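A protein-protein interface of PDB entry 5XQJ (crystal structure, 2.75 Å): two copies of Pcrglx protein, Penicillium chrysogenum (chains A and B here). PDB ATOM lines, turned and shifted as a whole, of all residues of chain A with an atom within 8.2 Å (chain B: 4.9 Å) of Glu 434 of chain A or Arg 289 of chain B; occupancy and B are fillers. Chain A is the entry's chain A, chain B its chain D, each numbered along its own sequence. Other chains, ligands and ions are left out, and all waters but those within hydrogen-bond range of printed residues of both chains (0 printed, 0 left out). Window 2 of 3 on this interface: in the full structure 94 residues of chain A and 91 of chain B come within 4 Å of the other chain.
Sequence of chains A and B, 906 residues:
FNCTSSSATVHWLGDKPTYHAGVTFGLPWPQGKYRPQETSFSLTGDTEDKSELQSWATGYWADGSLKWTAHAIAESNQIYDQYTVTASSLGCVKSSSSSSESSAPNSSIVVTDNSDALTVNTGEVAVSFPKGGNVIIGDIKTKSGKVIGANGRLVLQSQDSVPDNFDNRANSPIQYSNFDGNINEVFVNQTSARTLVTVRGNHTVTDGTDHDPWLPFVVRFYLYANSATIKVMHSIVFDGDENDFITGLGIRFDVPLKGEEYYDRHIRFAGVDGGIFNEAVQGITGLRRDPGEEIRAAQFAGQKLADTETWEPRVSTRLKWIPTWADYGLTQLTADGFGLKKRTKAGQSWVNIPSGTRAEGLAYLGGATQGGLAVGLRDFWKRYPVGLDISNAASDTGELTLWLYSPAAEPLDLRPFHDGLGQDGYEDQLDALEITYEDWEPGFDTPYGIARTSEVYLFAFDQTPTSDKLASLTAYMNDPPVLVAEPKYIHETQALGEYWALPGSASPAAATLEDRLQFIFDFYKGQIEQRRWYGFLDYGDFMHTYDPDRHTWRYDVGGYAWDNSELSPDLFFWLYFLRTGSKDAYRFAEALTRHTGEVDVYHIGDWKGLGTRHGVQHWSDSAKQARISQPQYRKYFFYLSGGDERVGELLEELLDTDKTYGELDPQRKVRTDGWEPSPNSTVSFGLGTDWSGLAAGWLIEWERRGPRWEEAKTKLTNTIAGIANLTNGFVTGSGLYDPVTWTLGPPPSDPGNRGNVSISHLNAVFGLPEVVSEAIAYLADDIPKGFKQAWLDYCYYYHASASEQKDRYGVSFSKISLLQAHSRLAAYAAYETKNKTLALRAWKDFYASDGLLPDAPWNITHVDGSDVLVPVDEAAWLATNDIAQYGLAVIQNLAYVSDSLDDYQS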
ATOM      1  N   GLU A 427      15.981 -22.297  35.258  1.00  0.00           N
ATOM      2  CA  GLU A 427      16.067 -23.611  34.665  1.00  0.00           C
ATOM      3  C   GLU A 427      14.749 -23.963  33.934  1.00  0.00           C
ATOM      4  O   GLU A 427      14.767 -24.399  32.783  1.00  0.00           O
ATOM      5  CB  GLU A 427      16.430 -24.667  35.720  1.00  0.00           C
ATOM      6  CG  GLU A 427      17.233 -25.837  35.143  1.00  0.00           C
ATOM      7  CD  GLU A 427      17.118 -27.158  35.911  1.00  0.00           C
ATOM      8  OE1 GLU A 427      16.434 -27.258  36.957  1.00  0.00           O
ATOM      9  OE2 GLU A 427      17.735 -28.126  35.440  1.00  0.00           O
ATOM     10  N   ASP A 428      13.615 -23.759  34.587  1.00  0.00           N
ATOM     11  CA  ASP A 428      12.313 -23.956  33.943  1.00  0.00           C
ATOM     12  C   ASP A 428      12.081 -23.000  32.771  1.00  0.00           C
ATOM     13  O   ASP A 428      11.504 -23.406  31.772  1.00  0.00           O
ATOM     14  CB  ASP A 428      11.144 -23.794  34.946  1.00  0.00           C
ATOM     15  CG  ASP A 428      10.991 -24.972  35.882  1.00  0.00           C
ATOM     16  OD1 ASP A 428      11.515 -26.069  35.548  1.00  0.00           O
ATOM     17  OD2 ASP A 428      10.317 -24.798  36.940  1.00  0.00           O
ATOM     18  N   GLN A 429      12.527 -21.747  32.886  1.00  0.00           N
ATOM     19  CA  GLN A 429      12.304 -20.744  31.844  1.00  0.00           C
ATOM     20  C   GLN A 429      13.059 -21.108  30.575  1.00  0.00           C
ATOM     21  O   GLN A 429      12.496 -21.055  29.487  1.00  0.00           O
ATOM     22  CB  GLN A 429      12.713 -19.347  32.318  1.00  0.00           C
ATOM     23  CG  GLN A 429      11.883 -18.828  33.490  1.00  0.00           C
ATOM     24  CD  GLN A 429      12.584 -17.779  34.328  1.00  0.00           C
ATOM     25  OE1 GLN A 429      13.665 -17.268  33.988  1.00  0.00           O
ATOM     26  NE2 GLN A 429      11.962 -17.444  35.438  1.00  0.00           N
ATOM     27  N   LEU A 430      14.306 -21.535  30.744  1.00  0.00           N
ATOM     28  CA  LEU A 430      15.151 -21.967  29.634  1.00  0.00           C
ATOM     29  C   LEU A 430      14.733 -23.271  28.993  1.00  0.00           C
ATOM     30  O   LEU A 430      15.087 -23.552  27.839  1.00  0.00           O
ATOM     31  CB  LEU A 430      16.604 -22.095  30.101  1.00  0.00           C
ATOM     32  CG  LEU A 430      17.300 -20.758  30.414  1.00  0.00           C
ATOM     33  CD1 LEU A 430      18.647 -21.028  31.071  1.00  0.00           C
ATOM     34  CD2 LEU A 430      17.451 -19.925  29.143  1.00  0.00           C
ATOM     35  N   ASP A 431      14.036 -24.089  29.757  1.00  0.00           N
ATOM     36  CA  ASP A 431      13.515 -25.348  29.249  1.00  0.00           C
ATOM     37  C   ASP A 431      12.222 -25.121  28.435  1.00  0.00           C
ATOM     38  O   ASP A 431      11.929 -25.882  27.502  1.00  0.00           O
ATOM     39  CB  ASP A 431      13.271 -26.317  30.424  1.00  0.00           C
ATOM     40  CG  ASP A 431      12.927 -27.723  29.972  1.00  0.00           C
ATOM     41  OD1 ASP A 431      13.718 -28.319  29.195  1.00  0.00           O
ATOM     42  OD2 ASP A 431      11.855 -28.214  30.399  1.00  0.00           O
ATOM     43  N   ALA A 432      11.451 -24.088  28.792  1.00  0.00           N
ATOM     44  CA  ALA A 432      10.304 -23.674  27.979  1.00  0.00           C
ATOM     45  C   ALA A 432      10.766 -22.987  26.668  1.00  0.00           C
ATOM     46  O   ALA A 432      10.128 -23.099  25.616  1.00  0.00           O
ATOM     47  CB  ALA A 432       9.433 -22.743  28.793  1.00  0.00           C
ATOM     48  N   LEU A 433      11.888 -22.272  26.752  1.00  0.00           N
ATOM     49  CA  LEU A 433      12.562 -21.719  25.568  1.00  0.00           C
ATOM     50  C   LEU A 433      12.868 -22.754  24.529  1.00  0.00           C
ATOM     51  O   LEU A 433      12.762 -22.451  23.367  1.00  0.00           O
ATOM     52  CB  LEU A 433      13.867 -21.013  25.932  1.00  0.00           C
ATOM     53  CG  LEU A 433      14.613 -20.242  24.847  1.00  0.00           C
ATOM     54  CD1 LEU A 433      13.771 -19.067  24.406  1.00  0.00           C
ATOM     55  CD2 LEU A 433      15.952 -19.761  25.396  1.00  0.00           C
ATOM     56  N   GLU A 434      13.227 -23.961  24.958  1.00  0.00           N
ATOM     57  CA  GLU A 434      13.523 -25.078  24.063  1.00  0.00           C
ATOM     58  C   GLU A 434      12.332 -25.580  23.249  1.00  0.00           C
ATOM     59  O   GLU A 434      12.578 -26.223  22.212  1.00  0.00           O
ATOM     60  CB  GLU A 434      14.180 -26.264  24.798  1.00  0.00           C
ATOM     61  CG  GLU A 434      15.653 -26.080  25.196  1.00  0.00           C
ATOM     62  CD  GLU A 434      16.622 -25.843  24.018  1.00  0.00           C
ATOM     63  OE1 GLU A 434      16.354 -26.304  22.864  1.00  0.00           O
ATOM     64  OE2 GLU A 434      17.676 -25.185  24.251  1.00  0.00           O
ATOM     65  N   ILE A 435      11.085 -25.270  23.659  1.00  0.00           N
ATOM     66  CA  ILE A 435       9.874 -25.729  22.924  1.00  0.00           C
ATOM     67  C   ILE A 435       8.972 -24.672  22.268  1.00  0.00           C
ATOM     68  O   ILE A 435       8.457 -24.902  21.149  1.00  0.00           O
ATOM     69  CB  ILE A 435       9.003 -26.674  23.777  1.00  0.00           C
ATOM     70  CG1 ILE A 435       7.930 -27.356  22.915  1.00  0.00           C
ATOM     71  CG2 ILE A 435       8.317 -25.954  24.926  1.00  0.00           C
ATOM     72  CD1 ILE A 435       8.539 -28.178  21.815  1.00  0.00           C
ATOM     73  N   THR A 436       8.710 -23.566  22.950  1.00  0.00           N
ATOM     74  CA  THR A 436       7.944 -22.478  22.307  1.00  0.00           C
ATOM     75  C   THR A 436       8.818 -21.331  21.804  1.00  0.00           C
ATOM     76  O   THR A 436       8.313 -20.506  21.080  1.00  0.00           O
ATOM     77  CB  THR A 436       6.903 -21.856  23.239  1.00  0.00           C
ATOM     78  OG1 THR A 436       7.581 -21.275  24.337  1.00  0.00           O
ATOM     79  CG2 THR A 436       5.951 -22.891  23.743  1.00  0.00           C
ATOM     80  N   TYR A 437      10.097 -21.282  22.209  1.00  0.00           N
ATOM     81  CA  TYR A 437      11.050 -20.192  21.862  1.00  0.00           C
ATOM     82  C   TYR A 437      10.754 -18.897  22.626  1.00  0.00           C
ATOM     83  O   TYR A 437      11.193 -17.847  22.215  1.00  0.00           O
ATOM     84  CB  TYR A 437      11.134 -19.949  20.312  1.00  0.00           C
ATOM     85  CG  TYR A 437      12.474 -19.481  19.691  1.00  0.00           C
ATOM     86  CD1 TYR A 437      13.712 -19.958  20.133  1.00  0.00           C
ATOM     87  CD2 TYR A 437      12.470 -18.622  18.591  1.00  0.00           C
ATOM     88  CE1 TYR A 437      14.901 -19.550  19.539  1.00  0.00           C
ATOM     89  CE2 TYR A 437      13.658 -18.216  17.974  1.00  0.00           C
ATOM     90  CZ  TYR A 437      14.871 -18.672  18.453  1.00  0.00           C
ATOM     91  OH  TYR A 437      16.038 -18.250  17.828  1.00  0.00           O
ATOM     92  N   GLU A 438      10.049 -18.996  23.746  1.00  0.00           N
ATOM     93  CA  GLU A 438       9.781 -17.863  24.607  1.00  0.00           C
ATOM     94  C   GLU A 438      10.724 -17.889  25.791  1.00  0.00           C
ATOM     95  O   GLU A 438      11.030 -18.962  26.307  1.00  0.00           O
ATOM     96  CB  GLU A 438       8.366 -17.962  25.127  1.00  0.00           C
ATOM     97  CG  GLU A 438       7.901 -16.694  25.819  1.00  0.00           C
ATOM     98  CD  GLU A 438       6.517 -16.827  26.368  1.00  0.00           C
ATOM     99  OE1 GLU A 438       6.346 -17.744  27.196  1.00  0.00           O
ATOM    100  OE2 GLU A 438       5.641 -16.018  25.977  1.00  0.00           O
ATOM    101  N   ASP A 439      11.180 -16.726  26.234  1.00  0.00           N
ATOM    102  CA  ASP A 439      12.038 -16.661  27.403  1.00  0.00           C
ATOM    103  C   ASP A 439      11.228 -15.977  28.475  1.00  0.00           C
ATOM    104  O   ASP A 439      11.242 -14.759  28.614  1.00  0.00           O
ATOM    105  CB  ASP A 439      13.357 -15.910  27.090  1.00  0.00           C
ATOM    106  CG  ASP A 439      14.415 -16.087  28.179  1.00  0.00           C
ATOM    107  OD1 ASP A 439      14.133 -16.845  29.112  1.00  0.00           O
ATOM    108  OD2 ASP A 439      15.512 -15.486  28.112  1.00  0.00           O
ATOM    109  N   ARG A 554       2.976 -18.313  13.285  1.00  0.00           N
ATOM    110  CA  ARG A 554       2.860 -18.852  14.636  1.00  0.00           C
ATOM    111  C   ARG A 554       2.542 -17.743  15.649  1.00  0.00           C
ATOM    112  O   ARG A 554       3.362 -17.397  16.514  1.00  0.00           O
ATOM    113  CB  ARG A 554       4.115 -19.596  15.025  1.00  0.00           C
ATOM    114  CG  ARG A 554       4.478 -20.735  14.094  1.00  0.00           C
ATOM    115  CD  ARG A 554       5.942 -21.098  14.309  1.00  0.00           C
ATOM    116  NE  ARG A 554       6.373 -22.259  13.513  1.00  0.00           N
ATOM    117  CZ  ARG A 554       7.477 -22.959  13.736  1.00  0.00           C
ATOM    118  NH1 ARG A 554       8.289 -22.690  14.732  1.00  0.00           N
ATOM    119  NH2 ARG A 554       7.746 -23.940  12.964  1.00  0.00           N
ATOM    120  N   VAL A 557       2.604 -19.038  19.482  1.00  0.00           N
ATOM    121  CA  VAL A 557       3.691 -19.879  19.987  1.00  0.00           C
ATOM    122  C   VAL A 557       4.928 -19.068  20.259  1.00  0.00           C
ATOM    123  O   VAL A 557       5.631 -18.660  19.346  1.00  0.00           O
ATOM    124  CB  VAL A 557       4.044 -20.986  19.003  1.00  0.00           C
ATOM    125  CG1 VAL A 557       5.111 -21.913  19.586  1.00  0.00           C
ATOM    126  CG2 VAL A 557       2.786 -21.760  18.629  1.00  0.00           C
ATOM    127  N   TYR A 560       7.802 -17.156  17.985  1.00  0.00           N
ATOM    128  CA  TYR A 560       7.525 -17.246  16.572  1.00  0.00           C
ATOM    129  C   TYR A 560       6.409 -16.304  16.076  1.00  0.00           C
ATOM    130  O   TYR A 560       6.123 -16.268  14.883  1.00  0.00           O
ATOM    131  CB  TYR A 560       7.209 -18.686  16.242  1.00  0.00           C
ATOM    132  CG  TYR A 560       8.328 -19.615  16.548  1.00  0.00           C
ATOM    133  CD1 TYR A 560       9.567 -19.481  15.906  1.00  0.00           C
ATOM    134  CD2 TYR A 560       8.166 -20.654  17.429  1.00  0.00           C
ATOM    135  CE1 TYR A 560      10.609 -20.358  16.142  1.00  0.00           C
ATOM    136  CE2 TYR A 560       9.213 -21.533  17.693  1.00  0.00           C
ATOM    137  CZ  TYR A 560      10.428 -21.377  17.048  1.00  0.00           C
ATOM    138  OH  TYR A 560      11.452 -22.237  17.320  1.00  0.00           O
ATOM    139  N   LEU B 287       5.882 -25.728  16.629  1.00  0.00           N
ATOM    140  CA  LEU B 287       6.770 -25.611  17.790  1.00  0.00           C
ATOM    141  C   LEU B 287       8.203 -25.515  17.325  1.00  0.00           C
ATOM    142  O   LEU B 287       8.503 -25.719  16.142  1.00  0.00           O
ATOM    143  CB  LEU B 287       6.639 -26.836  18.693  1.00  0.00           C
ATOM    144  CG  LEU B 287       5.260 -27.160  19.249  1.00  0.00           C
ATOM    145  CD1 LEU B 287       5.292 -28.534  19.926  1.00  0.00           C
ATOM    146  CD2 LEU B 287       4.818 -26.066  20.208  1.00  0.00           C
ATOM    147  N   ARG B 288       9.083 -25.244  18.281  1.00  0.00           N
ATOM    148  CA  ARG B 288      10.502 -25.217  18.037  1.00  0.00           C
ATOM    149  C   ARG B 288      11.047 -26.580  17.692  1.00  0.00           C
ATOM    150  O   ARG B 288      11.947 -26.695  16.894  1.00  0.00           O
ATOM    151  CB  ARG B 288      11.202 -24.732  19.253  1.00  0.00           C
ATOM    152  CG  ARG B 288      12.681 -24.592  19.027  1.00  0.00           C
ATOM    153  CD  ARG B 288      13.314 -23.645  20.030  1.00  0.00           C
ATOM    154  NE  ARG B 288      14.689 -23.466  19.630  1.00  0.00           N
ATOM    155  CZ  ARG B 288      15.671 -23.021  20.401  1.00  0.00           C
ATOM    156  NH1 ARG B 288      15.492 -22.667  21.668  1.00  0.00           N
ATOM    157  NH2 ARG B 288      16.871 -22.936  19.867  1.00  0.00           N
ATOM    158  N   ARG B 289      10.481 -27.612  18.296  1.00  0.00           N
ATOM    159  CA  ARG B 289      10.865 -28.986  18.030  1.00  0.00           C
ATOM    160  C   ARG B 289       9.718 -29.745  17.352  1.00  0.00           C
ATOM    161  O   ARG B 289       8.548 -29.383  17.477  1.00  0.00           O
ATOM    162  CB  ARG B 289      11.263 -29.648  19.343  1.00  0.00           C
ATOM    163  CG  ARG B 289      12.524 -29.083  19.966  1.00  0.00           C
ATOM    164  CD  ARG B 289      13.776 -29.739  19.417  1.00  0.00           C
ATOM    165  NE  ARG B 289      14.870 -28.764  19.313  1.00  0.00           N
ATOM    166  CZ  ARG B 289      15.282 -28.155  18.200  1.00  0.00           C
ATOM    167  NH1 ARG B 289      14.720 -28.400  17.022  1.00  0.00           N
ATOM    168  NH2 ARG B 289      16.275 -27.271  18.273  1.00  0.00           N
ATOM    169  N   ASP B 290      10.084 -30.797  16.625  1.00  0.00           N
ATOM    170  CA  ASP B 290       9.181 -31.506  15.738  1.00  0.00           C
ATOM    171  C   ASP B 290       8.855 -32.808  16.450  1.00  0.00           C
ATOM    172  O   ASP B 290       9.729 -33.621  16.699  1.00  0.00           O
ATOM    173  CB  ASP B 290       9.860 -31.737  14.381  1.00  0.00           C
ATOM    174  CG  ASP B 290       8.920 -32.323  13.288  1.00  0.00           C
ATOM    175  OD1 ASP B 290       7.729 -32.658  13.530  1.00  0.00           O
ATOM    176  OD2 ASP B 290       9.405 -32.438  12.131  1.00  0.00           O
ATOM    177  N   PRO B 291       7.594 -32.992  16.837  1.00  0.00           N
ATOM    178  CA  PRO B 291       7.267 -34.255  17.481  1.00  0.00           C
ATOM    179  C   PRO B 291       7.304 -35.382  16.478  1.00  0.00           C
ATOM    180  O   PRO B 291       7.553 -36.512  16.850  1.00  0.00           O
ATOM    181  CB  PRO B 291       5.841 -34.029  17.981  1.00  0.00           C
ATOM    182  CG  PRO B 291       5.262 -33.082  16.970  1.00  0.00           C
ATOM    183  CD  PRO B 291       6.400 -32.148  16.632  1.00  0.00           C
ATOM    184  N   ARG B 314      12.274 -34.557  22.887  1.00  0.00           N
ATOM    185  CA  ARG B 314      12.492 -33.125  23.091  1.00  0.00           C
ATOM    186  C   ARG B 314      11.169 -32.341  23.041  1.00  0.00           C
ATOM    187  O   ARG B 314      11.135 -31.207  23.535  1.00  0.00           O
ATOM    188  CB  ARG B 314      13.517 -32.565  22.097  1.00  0.00           C
ATOM    189  CG  ARG B 314      14.960 -32.946  22.430  1.00  0.00           C
ATOM    190  CD  ARG B 314      15.934 -32.383  21.399  1.00  0.00           C
ATOM    191  NE  ARG B 314      15.582 -32.838  20.044  1.00  0.00           N
ATOM    192  CZ  ARG B 314      16.060 -32.339  18.899  1.00  0.00           C
ATOM    193  NH1 ARG B 314      16.954 -31.346  18.894  1.00  0.00           N
ATOM    194  NH2 ARG B 314      15.626 -32.846  17.746  1.00  0.00           N
ATOM    195  N   VAL B 315      10.112 -32.936  22.453  1.00  0.00           N
ATOM    196  CA  VAL B 315       8.760 -32.394  22.529  1.00  0.00           C
ATOM    197  C   VAL B 315       7.882 -32.947  23.672  1.00  0.00           C
ATOM    198  O   VAL B 315       7.292 -32.184  24.440  1.00  0.00           O
ATOM    199  CB  VAL B 315       8.003 -32.641  21.232  1.00  0.00           C
ATOM    200  CG1 VAL B 315       6.534 -32.149  21.346  1.00  0.00           C
ATOM    201  CG2 VAL B 315       8.734 -31.973  20.080  1.00  0.00           C
ATOM    202  N   ARG B 318       8.089 -31.930  27.257  1.00  0.00           N
ATOM    203  CA  ARG B 318       7.924 -30.498  27.474  1.00  0.00           C
ATOM    204  C   ARG B 318       6.508 -29.972  27.296  1.00  0.00           C
ATOM    205  O   ARG B 318       6.310 -28.766  27.235  1.00  0.00           O
ATOM    206  CB  ARG B 318       8.880 -29.751  26.548  1.00  0.00           C
ATOM    207  CG  ARG B 318      10.331 -30.014  26.882  1.00  0.00           C
ATOM    208  CD  ARG B 318      11.169 -28.914  26.310  1.00  0.00           C
ATOM    209  NE  ARG B 318      12.572 -28.965  26.716  1.00  0.00           N
ATOM    210  CZ  ARG B 318      13.565 -29.521  26.012  1.00  0.00           C
ATOM    211  NH1 ARG B 318      13.354 -30.136  24.836  1.00  0.00           N
ATOM    212  NH2 ARG B 318      14.804 -29.448  26.492  1.00  0.00           N
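No position is printed for both chains.
Of the 11 pairs that touch across the chains among the printed residues, none has its exchanged pair printed and touching as well.
Among the printed residues, pairs that only touch across the chains: Glu 434 of chain A with Arg 289 of chain B, Glu 434 of chain A with Arg 318 of chain B, Ile 435 of chain A with Leu 287 of chain B, Ile 435 of chain A with Arg 289 of chain B, Tyr 437 of chain A with Arg 288 of chain B and Tyr 560 of chain A with Arg 288 of chain B.
Of the 8 printed residues of chain B, 4 touch a printed residue of chain A.
Printed residues of chain B that touch a printed residue of chain A: Leu 287, Arg 288, Arg 289 and Arg 318.
Hydrophobic or aromatic side chains of chain B within 4 Å of the printed part of chain A: Leu 287.
Along chain B the printed residues that touch a printed residue of chain A span positions 287 to 318.
Of the 16 printed residues of chain A, 7 touch a printed residue of chain B.
Printed residues of chain A that touch a printed residue of chain B: Asp 431, Leu 433, Glu 434, Ile 435, Tyr 437, Arg 554 and Tyr 560.
Hydrophobic or aromatic side chains of chain A that line the printed part of chain B: Ile 435, Tyr 437 and Tyr 560.
Glu 434 of chain A touches just these residues of chain B: Arg 288, Arg 289 and Arg 318.
Of chain A, only Glu 434 and Ile 435 come within 4 Å of Arg 289 of chain B.
Of the printed residues of chain A, Leu 287 of chain B touches Ile 435 and Arg 554.
Printed residues of chain A within 4 Å of Arg 318 of chain B: Asp 431 and Glu 434.
Of the printed residues of chain B, Tyr 560 of chain A touches Arg 288 (3.2 Å).
Arg 314 of chain B touches none of the printed residues of chain A.
The nearest residue of chain A that does not touch Arg 289 of chain B is Tyr 560 of chain A (5.5 Å).
The backbone carbonyl oxygen of Arg 314 of chain B is in hydrogen-bond range of the guanidinium group of Arg 318 of chain B (2.8 Å).
The backbone carbonyl oxygen (O) of Glu 438 of chain A sits close to the backbone NH (N) of Leu 433 of chain A, 3.4 Å away.
OD1 of Asp 431 of chain A lies within salt-bridge range of NE of Arg 318 of chain B, 2.8 Å away.
OE1 of Glu 434 of chain A is in salt-bridge range of NH1 of Arg 288 of chain B (3.9 Å).
The backbone carbonyl oxygen (O) of Leu 433 of chain A lies within hydrogen-bond range of the guanidinium group (NH1) of Arg 288 of chain B (3.2 Å).
NH1 of Arg 554 of chain A sits at hydrogen-bond distance from O of Leu 287 of chain B.
The backbone carbonyl oxygen of Ile 435 of chain A is in hydrogen-bond range of the backbone NH of Arg 288 of chain B.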
